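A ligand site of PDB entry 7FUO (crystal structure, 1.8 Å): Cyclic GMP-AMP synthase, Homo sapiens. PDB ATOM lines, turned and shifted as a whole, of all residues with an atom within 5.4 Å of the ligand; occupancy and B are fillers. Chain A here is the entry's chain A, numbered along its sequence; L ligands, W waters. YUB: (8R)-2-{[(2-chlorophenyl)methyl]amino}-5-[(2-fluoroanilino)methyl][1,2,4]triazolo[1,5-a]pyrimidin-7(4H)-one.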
ATOM      1  N   ALA A  87      -6.174   8.279  -0.548  1.00  0.00           N
ATOM      2  CA  ALA A  87      -6.331   9.655  -1.019  1.00  0.00           C
ATOM      3  C   ALA A  87      -5.855  10.717  -0.044  1.00  0.00           C
ATOM      4  O   ALA A  87      -5.642  11.849  -0.474  1.00  0.00           O
ATOM      5  CB  ALA A  87      -7.797   9.935  -1.362  1.00  0.00           C
ATOM      6  N   TYR A  88      -5.703  10.404   1.250  1.00  0.00           N
ATOM      7  CA  TYR A  88      -5.373  11.410   2.260  1.00  0.00           C
ATOM      8  C   TYR A  88      -3.983  11.177   2.847  1.00  0.00           C
ATOM      9  O   TYR A  88      -3.585  10.036   3.116  1.00  0.00           O
ATOM     10  CB  TYR A  88      -6.390  11.427   3.391  1.00  0.00           C
ATOM     11  CG  TYR A  88      -7.796  11.640   2.915  1.00  0.00           C
ATOM     12  CD1 TYR A  88      -8.543  10.585   2.401  1.00  0.00           C
ATOM     13  CD2 TYR A  88      -8.375  12.908   2.942  1.00  0.00           C
ATOM     14  CE1 TYR A  88      -9.851  10.781   1.941  1.00  0.00           C
ATOM     15  CE2 TYR A  88      -9.669  13.113   2.494  1.00  0.00           C
ATOM     16  CZ  TYR A  88     -10.406  12.045   1.996  1.00  0.00           C
ATOM     17  OH  TYR A  88     -11.684  12.244   1.550  1.00  0.00           O
ATOM     18  N   LEU A 178      -5.756   6.749 -14.158  1.00  0.00           N
ATOM     19  CA  LEU A 178      -5.636   7.522 -15.384  1.00  0.00           C
ATOM     20  C   LEU A 178      -5.497   6.574 -16.575  1.00  0.00           C
ATOM     21  O   LEU A 178      -4.582   6.682 -17.401  1.00  0.00           O
ATOM     22  CB  LEU A 178      -4.460   8.491 -15.302  1.00  0.00           C
ATOM     23  CG  LEU A 178      -4.414   9.639 -16.307  1.00  0.00           C
ATOM     24  CD1 LEU A 178      -5.722  10.395 -16.318  1.00  0.00           C
ATOM     25  CD2 LEU A 178      -3.287  10.551 -15.927  1.00  0.00           C
ATOM     26  N   ARG A 216      -5.693  16.001   0.999  1.00  0.00           N
ATOM     27  CA  ARG A 216      -6.287  15.133  -0.007  1.00  0.00           C
ATOM     28  C   ARG A 216      -5.685  15.392  -1.387  1.00  0.00           C
ATOM     29  O   ARG A 216      -5.487  16.545  -1.779  1.00  0.00           O
ATOM     30  CB  ARG A 216      -7.781  15.348  -0.072  1.00  0.00           C
ATOM     31  CG  ARG A 216      -8.449  14.277  -0.898  1.00  0.00           C
ATOM     32  CD  ARG A 216      -9.902  14.559  -0.962  1.00  0.00           C
ATOM     33  NE  ARG A 216     -10.114  15.774  -1.707  1.00  0.00           N
ATOM     34  CZ  ARG A 216     -11.258  16.449  -1.713  1.00  0.00           C
ATOM     35  NH1 ARG A 216     -11.350  17.553  -2.426  1.00  0.00           N
ATOM     36  NH2 ARG A 216     -12.295  16.005  -1.014  1.00  0.00           N
ATOM     37  N   LEU A 217      -5.403  14.312  -2.114  1.00  0.00           N
ATOM     38  CA  LEU A 217      -4.853  14.453  -3.457  1.00  0.00           C
ATOM     39  C   LEU A 217      -5.841  15.187  -4.332  1.00  0.00           C
ATOM     40  O   LEU A 217      -7.045  14.922  -4.271  1.00  0.00           O
ATOM     41  CB  LEU A 217      -4.542  13.091  -4.091  1.00  0.00           C
ATOM     42  CG  LEU A 217      -3.340  12.311  -3.587  1.00  0.00           C
ATOM     43  CD1 LEU A 217      -3.240  10.961  -4.308  1.00  0.00           C
ATOM     44  CD2 LEU A 217      -2.097  13.132  -3.838  1.00  0.00           C
ATOM     45  N   SER A 218      -5.343  16.122  -5.133  1.00  0.00           N
ATOM     46  CA  SER A 218      -6.163  16.828  -6.092  1.00  0.00           C
ATOM     47  C   SER A 218      -5.509  16.775  -7.461  1.00  0.00           C
ATOM     48  O   SER A 218      -4.295  16.932  -7.588  1.00  0.00           O
ATOM     49  CB  SER A 218      -6.374  18.293  -5.677  1.00  0.00           C
ATOM     50  OG  SER A 218      -6.953  19.041  -6.747  1.00  0.00           O
ATOM     51  N   PHE A 219      -6.330  16.536  -8.483  1.00  0.00           N
ATOM     52  CA  PHE A 219      -5.868  16.562  -9.871  1.00  0.00           C
ATOM     53  C   PHE A 219      -6.760  17.455 -10.710  1.00  0.00           C
ATOM     54  O   PHE A 219      -7.023  17.167 -11.884  1.00  0.00           O
ATOM     55  CB  PHE A 219      -5.840  15.146 -10.461  1.00  0.00           C
ATOM     56  CG  PHE A 219      -4.909  14.210  -9.729  1.00  0.00           C
ATOM     57  CD1 PHE A 219      -3.583  14.121 -10.090  1.00  0.00           C
ATOM     58  CD2 PHE A 219      -5.361  13.433  -8.676  1.00  0.00           C
ATOM     59  CE1 PHE A 219      -2.728  13.272  -9.425  1.00  0.00           C
ATOM     60  CE2 PHE A 219      -4.498  12.572  -8.012  1.00  0.00           C
ATOM     61  CZ  PHE A 219      -3.187  12.490  -8.377  1.00  0.00           C
ATOM     62  N   SER A 220      -7.252  18.548 -10.110  1.00  0.00           N
ATOM     63  CA  SER A 220      -8.218  19.413 -10.792  1.00  0.00           C
ATOM     64  C   SER A 220      -7.633  20.110 -12.004  1.00  0.00           C
ATOM     65  O   SER A 220      -8.371  20.828 -12.692  1.00  0.00           O
ATOM     66  CB  SER A 220      -8.751  20.459  -9.818  1.00  0.00           C
ATOM     67  OG  SER A 220      -7.717  21.316  -9.380  1.00  0.00           O
ATOM     68  N   HIS A 221      -6.342  19.986 -12.254  1.00  0.00           N
ATOM     69  CA  HIS A 221      -5.767  20.565 -13.445  1.00  0.00           C
ATOM     70  C   HIS A 221      -5.833  19.640 -14.647  1.00  0.00           C
ATOM     71  O   HIS A 221      -5.441  20.045 -15.749  1.00  0.00           O
ATOM     72  CB  HIS A 221      -4.319  20.966 -13.178  1.00  0.00           C
ATOM     73  CG  HIS A 221      -3.435  19.829 -12.770  1.00  0.00           C
ATOM     74  ND1 HIS A 221      -3.722  19.022 -11.685  1.00  0.00           N
ATOM     75  CD2 HIS A 221      -2.274  19.377 -13.291  1.00  0.00           C
ATOM     76  CE1 HIS A 221      -2.770  18.118 -11.565  1.00  0.00           C
ATOM     77  NE2 HIS A 221      -1.873  18.313 -12.516  1.00  0.00           N
ATOM     78  N   ILE A 222      -6.315  18.410 -14.468  1.00  0.00           N
ATOM     79  CA  ILE A 222      -6.180  17.399 -15.506  1.00  0.00           C
ATOM     80  C   ILE A 222      -7.359  17.434 -16.481  1.00  0.00           C
ATOM     81  O   ILE A 222      -7.168  17.222 -17.682  1.00  0.00           O
ATOM     82  CB  ILE A 222      -6.020  16.024 -14.855  1.00  0.00           C
ATOM     83  CG1 ILE A 222      -4.738  16.026 -14.011  1.00  0.00           C
ATOM     84  CG2 ILE A 222      -5.967  14.954 -15.923  1.00  0.00           C
ATOM     85  CD1 ILE A 222      -3.505  16.126 -14.821  1.00  0.00           C
ATOM     86  N   GLU A 223      -8.561  17.727 -15.955  1.00  0.00           N
ATOM     87  CA  GLU A 223      -9.766  17.799 -16.778  1.00  0.00           C
ATOM     88  C   GLU A 223      -9.564  18.729 -17.967  1.00  0.00           C
ATOM     89  O   GLU A 223      -9.901  18.387 -19.108  1.00  0.00           O
ATOM     90  CB  GLU A 223     -10.939  18.270 -15.923  1.00  0.00           C
ATOM     91  CG  GLU A 223     -12.317  18.242 -16.618  1.00  0.00           C
ATOM     92  CD  GLU A 223     -13.458  18.907 -15.804  1.00  0.00           C
ATOM     93  OE1 GLU A 223     -13.232  19.254 -14.615  1.00  0.00           O
ATOM     94  OE2 GLU A 223     -14.572  19.087 -16.356  1.00  0.00           O
ATOM     95  N   ILE A 226      -7.533  17.152 -20.745  1.00  0.00           N
ATOM     96  CA  ILE A 226      -8.232  16.168 -21.532  1.00  0.00           C
ATOM     97  C   ILE A 226      -9.337  16.803 -22.355  1.00  0.00           C
ATOM     98  O   ILE A 226      -9.479  16.513 -23.554  1.00  0.00           O
ATOM     99  CB  ILE A 226      -8.753  15.071 -20.617  1.00  0.00           C
ATOM    100  CG1 ILE A 226      -7.572  14.224 -20.139  1.00  0.00           C
ATOM    101  CG2 ILE A 226      -9.782  14.229 -21.352  1.00  0.00           C
ATOM    102  CD1 ILE A 226      -7.933  13.228 -19.130  1.00  0.00           C
ATOM    103  N   TYR A 276     -17.978  15.940  -9.055  1.00  0.00           N
ATOM    104  CA  TYR A 276     -16.959  14.897  -9.034  1.00  0.00           C
ATOM    105  C   TYR A 276     -17.478  13.597  -9.619  1.00  0.00           C
ATOM    106  O   TYR A 276     -16.910  13.040 -10.555  1.00  0.00           O
ATOM    107  CB  TYR A 276     -16.529  14.596  -7.594  1.00  0.00           C
ATOM    108  CG  TYR A 276     -15.313  15.310  -7.181  1.00  0.00           C
ATOM    109  CD1 TYR A 276     -15.355  16.671  -6.879  1.00  0.00           C
ATOM    110  CD2 TYR A 276     -14.110  14.640  -7.088  1.00  0.00           C
ATOM    111  CE1 TYR A 276     -14.213  17.348  -6.483  1.00  0.00           C
ATOM    112  CE2 TYR A 276     -12.967  15.301  -6.699  1.00  0.00           C
ATOM    113  CZ  TYR A 276     -13.023  16.660  -6.395  1.00  0.00           C
ATOM    114  OH  TYR A 276     -11.909  17.332  -5.997  1.00  0.00           O
ATOM    115  N   LYS A 279     -18.434  13.748 -13.323  1.00  0.00           N
ATOM    116  CA  LYS A 279     -17.222  13.795 -14.134  1.00  0.00           C
ATOM    117  C   LYS A 279     -16.544  12.434 -14.174  1.00  0.00           C
ATOM    118  O   LYS A 279     -16.273  11.896 -15.256  1.00  0.00           O
ATOM    119  CB  LYS A 279     -16.251  14.859 -13.604  1.00  0.00           C
ATOM    120  CG  LYS A 279     -16.745  16.273 -13.796  1.00  0.00           C
ATOM    121  CD  LYS A 279     -15.676  17.302 -13.477  1.00  0.00           C
ATOM    122  CE  LYS A 279     -16.273  18.706 -13.431  1.00  0.00           C
ATOM    123  NZ  LYS A 279     -15.257  19.790 -13.201  1.00  0.00           N
ATOM    124  N   THR A 280     -16.260  11.865 -13.000  1.00  0.00           N
ATOM    125  CA  THR A 280     -15.610  10.566 -12.945  1.00  0.00           C
ATOM    126  C   THR A 280     -16.377   9.542 -13.757  1.00  0.00           C
ATOM    127  O   THR A 280     -15.771   8.726 -14.465  1.00  0.00           O
ATOM    128  CB  THR A 280     -15.490  10.072 -11.509  1.00  0.00           C
ATOM    129  OG1 THR A 280     -14.887  11.079 -10.710  1.00  0.00           O
ATOM    130  CG2 THR A 280     -14.594   8.856 -11.457  1.00  0.00           C
ATOM    131  N   PHE A 283     -15.841  10.357 -17.605  1.00  0.00           N
ATOM    132  CA  PHE A 283     -14.546   9.988 -18.170  1.00  0.00           C
ATOM    133  C   PHE A 283     -14.326   8.500 -18.169  1.00  0.00           C
ATOM    134  O   PHE A 283     -13.502   8.017 -18.946  1.00  0.00           O
ATOM    135  CB  PHE A 283     -13.418  10.706 -17.420  1.00  0.00           C
ATOM    136  CG  PHE A 283     -13.365  12.191 -17.719  1.00  0.00           C
ATOM    137  CD1 PHE A 283     -12.895  12.621 -18.945  1.00  0.00           C
ATOM    138  CD2 PHE A 283     -13.848  13.127 -16.829  1.00  0.00           C
ATOM    139  CE1 PHE A 283     -12.861  13.969 -19.269  1.00  0.00           C
ATOM    140  CE2 PHE A 283     -13.833  14.467 -17.141  1.00  0.00           C
ATOM    141  CZ  PHE A 283     -13.327  14.891 -18.371  1.00  0.00           C
ATOM    142  N   ASN A 322     -12.629   6.078  -8.370  1.00  0.00           N
ATOM    143  CA  ASN A 322     -11.977   7.341  -8.669  1.00  0.00           C
ATOM    144  C   ASN A 322     -11.055   7.136  -9.868  1.00  0.00           C
ATOM    145  O   ASN A 322     -10.505   6.053 -10.072  1.00  0.00           O
ATOM    146  CB  ASN A 322     -11.166   7.863  -7.485  1.00  0.00           C
ATOM    147  CG  ASN A 322     -10.471   9.162  -7.799  1.00  0.00           C
ATOM    148  OD1 ASN A 322      -9.367   9.177  -8.367  1.00  0.00           O
ATOM    149  ND2 ASN A 322     -11.121  10.267  -7.484  1.00  0.00           N
ATOM    150  N   TYR A 323     -10.934   8.180 -10.696  1.00  0.00           N
ATOM    151  CA  TYR A 323     -10.235   8.029 -11.966  1.00  0.00           C
ATOM    152  C   TYR A 323      -8.729   7.905 -11.791  1.00  0.00           C
ATOM    153  O   TYR A 323      -8.045   7.306 -12.637  1.00  0.00           O
ATOM    154  CB  TYR A 323     -10.514   9.215 -12.856  1.00  0.00           C
ATOM    155  CG  TYR A 323     -10.417   8.887 -14.300  1.00  0.00           C
ATOM    156  CD1 TYR A 323     -11.373   8.080 -14.901  1.00  0.00           C
ATOM    157  CD2 TYR A 323      -9.380   9.372 -15.089  1.00  0.00           C
ATOM    158  CE1 TYR A 323     -11.310   7.763 -16.235  1.00  0.00           C
ATOM    159  CE2 TYR A 323      -9.306   9.074 -16.435  1.00  0.00           C
ATOM    160  CZ  TYR A 323     -10.286   8.260 -16.998  1.00  0.00           C
ATOM    161  OH  TYR A 323     -10.235   7.933 -18.326  1.00  0.00           O
ATOM    162  N   PHE A 324      -8.199   8.492 -10.740  1.00  0.00           N
ATOM    163  CA  PHE A 324      -6.766   8.497 -10.542  1.00  0.00           C
ATOM    164  C   PHE A 324      -6.332   7.443  -9.560  1.00  0.00           C
ATOM    165  O   PHE A 324      -5.220   6.916  -9.674  1.00  0.00           O
ATOM    166  CB  PHE A 324      -6.319   9.874 -10.059  1.00  0.00           C
ATOM    167  CG  PHE A 324      -6.689  10.962 -11.005  1.00  0.00           C
ATOM    168  CD1 PHE A 324      -5.869  11.261 -12.075  1.00  0.00           C
ATOM    169  CD2 PHE A 324      -7.864  11.644 -10.867  1.00  0.00           C
ATOM    170  CE1 PHE A 324      -6.222  12.248 -12.977  1.00  0.00           C
ATOM    171  CE2 PHE A 324      -8.220  12.624 -11.741  1.00  0.00           C
ATOM    172  CZ  PHE A 324      -7.408  12.934 -12.809  1.00  0.00           C
ATOM    173  N   ILE A 325      -7.202   7.108  -8.615  1.00  0.00           N
ATOM    174  CA  ILE A 325      -6.932   6.142  -7.568  1.00  0.00           C
ATOM    175  C   ILE A 325      -8.041   5.108  -7.645  1.00  0.00           C
ATOM    176  O   ILE A 325      -9.047   5.216  -6.921  1.00  0.00           O
ATOM    177  CB  ILE A 325      -6.839   6.799  -6.191  1.00  0.00           C
ATOM    178  CG1 ILE A 325      -5.672   7.781  -6.183  1.00  0.00           C
ATOM    179  CG2 ILE A 325      -6.534   5.789  -5.151  1.00  0.00           C
ATOM    180  CD1 ILE A 325      -5.949   8.980  -5.378  1.00  0.00           C
ATOM    181  N   PHE A 328     -10.084   3.530  -4.752  1.00  0.00           N
ATOM    182  CA  PHE A 328     -10.967   4.357  -3.931  1.00  0.00           C
ATOM    183  C   PHE A 328     -12.338   4.401  -4.587  1.00  0.00           C
ATOM    184  O   PHE A 328     -12.478   4.918  -5.699  1.00  0.00           O
ATOM    185  CB  PHE A 328     -10.408   5.775  -3.778  1.00  0.00           C
ATOM    186  CG  PHE A 328     -11.168   6.601  -2.802  1.00  0.00           C
ATOM    187  CD1 PHE A 328     -12.386   7.154  -3.147  1.00  0.00           C
ATOM    188  CD2 PHE A 328     -10.681   6.825  -1.552  1.00  0.00           C
ATOM    189  CE1 PHE A 328     -13.094   7.900  -2.263  1.00  0.00           C
ATOM    190  CE2 PHE A 328     -11.402   7.590  -0.631  1.00  0.00           C
ATOM    191  CZ  PHE A 328     -12.618   8.112  -0.990  1.00  0.00           C
ATOM    192  N   LEU A 330     -15.768   5.910  -4.876  1.00  0.00           N
ATOM    193  CA  LEU A 330     -16.553   7.077  -4.530  1.00  0.00           C
ATOM    194  C   LEU A 330     -17.950   6.694  -4.044  1.00  0.00           C
ATOM    195  O   LEU A 330     -18.506   7.395  -3.210  1.00  0.00           O
ATOM    196  CB  LEU A 330     -16.664   8.035  -5.723  1.00  0.00           C
ATOM    197  CG  LEU A 330     -15.331   8.568  -6.273  1.00  0.00           C
ATOM    198  CD1 LEU A 330     -15.604   9.400  -7.463  1.00  0.00           C
ATOM    199  CD2 LEU A 330     -14.578   9.385  -5.248  1.00  0.00           C
HETATM  200  C15 YUB L   1      -8.293  11.854  -5.844  1.00  0.00           C
HETATM  201  C16 YUB L   1      -9.921  10.693  -4.242  1.00  0.00           C
HETATM  202  C17 YUB L   1     -11.622  12.439 -14.404  1.00  0.00           C
HETATM  203  C18 YUB L   1     -12.993  14.371 -11.551  1.00  0.00           C
HETATM  204  C21 YUB L   1     -10.207  13.023  -4.652  1.00  0.00           C
HETATM  205  C22 YUB L   1     -11.033  14.639 -13.696  1.00  0.00           C
HETATM  206  C23 YUB L   1     -11.015  10.704  -3.393  1.00  0.00           C
HETATM  207  C24 YUB L   1     -10.703  12.482 -15.422  1.00  0.00           C
HETATM  208  C25 YUB L   1     -11.309  13.029  -3.808  1.00  0.00           C
HETATM  209  C26 YUB L   1      -9.949  13.623 -15.584  1.00  0.00           C
HETATM  210  C27 YUB L   1     -11.714  11.878  -3.184  1.00  0.00           C
HETATM  211  C28 YUB L   1     -10.110  14.696 -14.731  1.00  0.00           C
HETATM  212  C12 YUB L   1      -9.477  11.860  -4.892  1.00  0.00           C
HETATM  213  C14 YUB L   1     -11.807  13.491 -13.521  1.00  0.00           C
HETATM  214  C2  YUB L   1     -10.464  13.765  -8.849  1.00  0.00           C
HETATM  215  C5  YUB L   1     -10.326  16.112  -9.514  1.00  0.00           C
HETATM  216  C6  YUB L   1      -9.006  13.739  -7.357  1.00  0.00           C
HETATM  217  C7  YUB L   1     -11.338  15.818 -10.444  1.00  0.00           C
HETATM  218  C9  YUB L   1     -11.890  14.580 -10.555  1.00  0.00           C
HETATM  219  F20 YUB L   1     -12.381  11.339 -14.232  1.00  0.00           F
HETATM  220  N1  YUB L   1      -9.941  15.008  -8.740  1.00  0.00           N
HETATM  221  N10 YUB L   1      -8.157  13.226  -6.341  1.00  0.00           N
HETATM  222  N11 YUB L   1     -12.706  13.349 -12.518  1.00  0.00           N
HETATM  223  N3  YUB L   1      -9.907  12.925  -7.988  1.00  0.00           N
HETATM  224  N4  YUB L   1      -8.952  14.997  -7.761  1.00  0.00           N
HETATM  225  N8  YUB L   1     -11.447  13.536  -9.760  1.00  0.00           N
HETATM  226  O13 YUB L   1      -9.780  17.214  -9.372  1.00  0.00           O
HETATM  227 CL19 YUB L   1      -9.094   9.208  -4.481  1.00  0.00          CL
HETATM  228  O   HOH W   1      -9.282  18.163  -6.602  1.00  0.00           O
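Water W1 lies within hydrogen-bond range of OG of Ser 218 (2.5 Å), OH of Tyr 276 (2.8 Å) and O13 of the ligand (3.0 Å).
A nitrogen (N10) of the ligand sits at hydrogen-bond distance from the backbone carbonyl oxygen (O) of Leu 217. N of Ser 220 sits at hydrogen-bond distance from O13 of the ligand, at 3.0 Å. A nitrogen (N3) of the ligand lies within hydrogen-bond range of the side-chain amide nitrogen of Asn 322, at 3.0 Å. The backbone NH (N) of Phe 219 lies within hydrogen-bond range of a nitrogen (N4) of the ligand.
Ala 87 touches the ligand (CB to CL19, 3.5 Å). CD of Arg 216 touches C25 of the ligand (3.5 Å). CA of Ser 218 touches N4 of the ligand, 3.7 Å away. Glu 223 touches the ligand (N to C28, 3.6 Å). Tyr 276 touches the ligand (CE2 to C2, 3.6 Å). Lys 279 touches the ligand. Thr 280 touches the ligand. CD2 of Phe 283 touches C17 of the ligand, at 3.4 Å. Tyr 323 touches the ligand. CZ of Phe 324 touches C28 of the ligand, 3.8 Å away. CD1 of Ile 325 touches CL19 of the ligand, 3.3 Å away. CE1 of Phe 328 touches C23 of the ligand, at 3.7 Å. Hydrophobic or aromatic side chains that line the ligand: Ala 87, Phe 219, Tyr 276, Phe 283, Tyr 323, Phe 324, Ile 325 and Phe 328. Within 4 Å of the ligand: Ala 87, Arg 216, Leu 217, Ser 218, Phe 219, Ser 220, Glu 223, Tyr 276, Lys 279, Thr 280, Phe 283, Asn 322, Tyr 323, Phe 324, Ile 325 and Phe 328. Along chain A the residues within 4 Å of the ligand span positions 87 to 328. The nearest printed residue that does not touch the ligand is Ile 226 (4.1 Å).
The backbone carbonyl oxygen of Ala 87 is in hydrogen-bond range of the backbone NH of Leu 217. OG of Ser 218 sits at hydrogen-bond distance from N of Ser 220, at 3.4 Å. OD1 of Asn 322 is in hydrogen-bond range of N of Ile 325 (3.0 Å). The backbone carbonyl oxygen (O) of Phe 328 lies within hydrogen-bond range of the backbone NH (N) of Asn 322 (2.9 Å). OD1 of Asn 322 lies within hydrogen-bond range of N of Phe 324 (2.7 Å). The backbone carbonyl oxygen (O) of Tyr 323 is in hydrogen-bond range of the backbone NH (N) of Leu 178, at 2.8 Å. The side-chain hydroxyl (OG1) of Thr 280 is in hydrogen-bond range of the backbone carbonyl oxygen (O) of Tyr 276 (2.8 Å). The side-chain carboxylate of Glu 223 is in salt-bridge range of the side-chain amino group of Lys 279.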
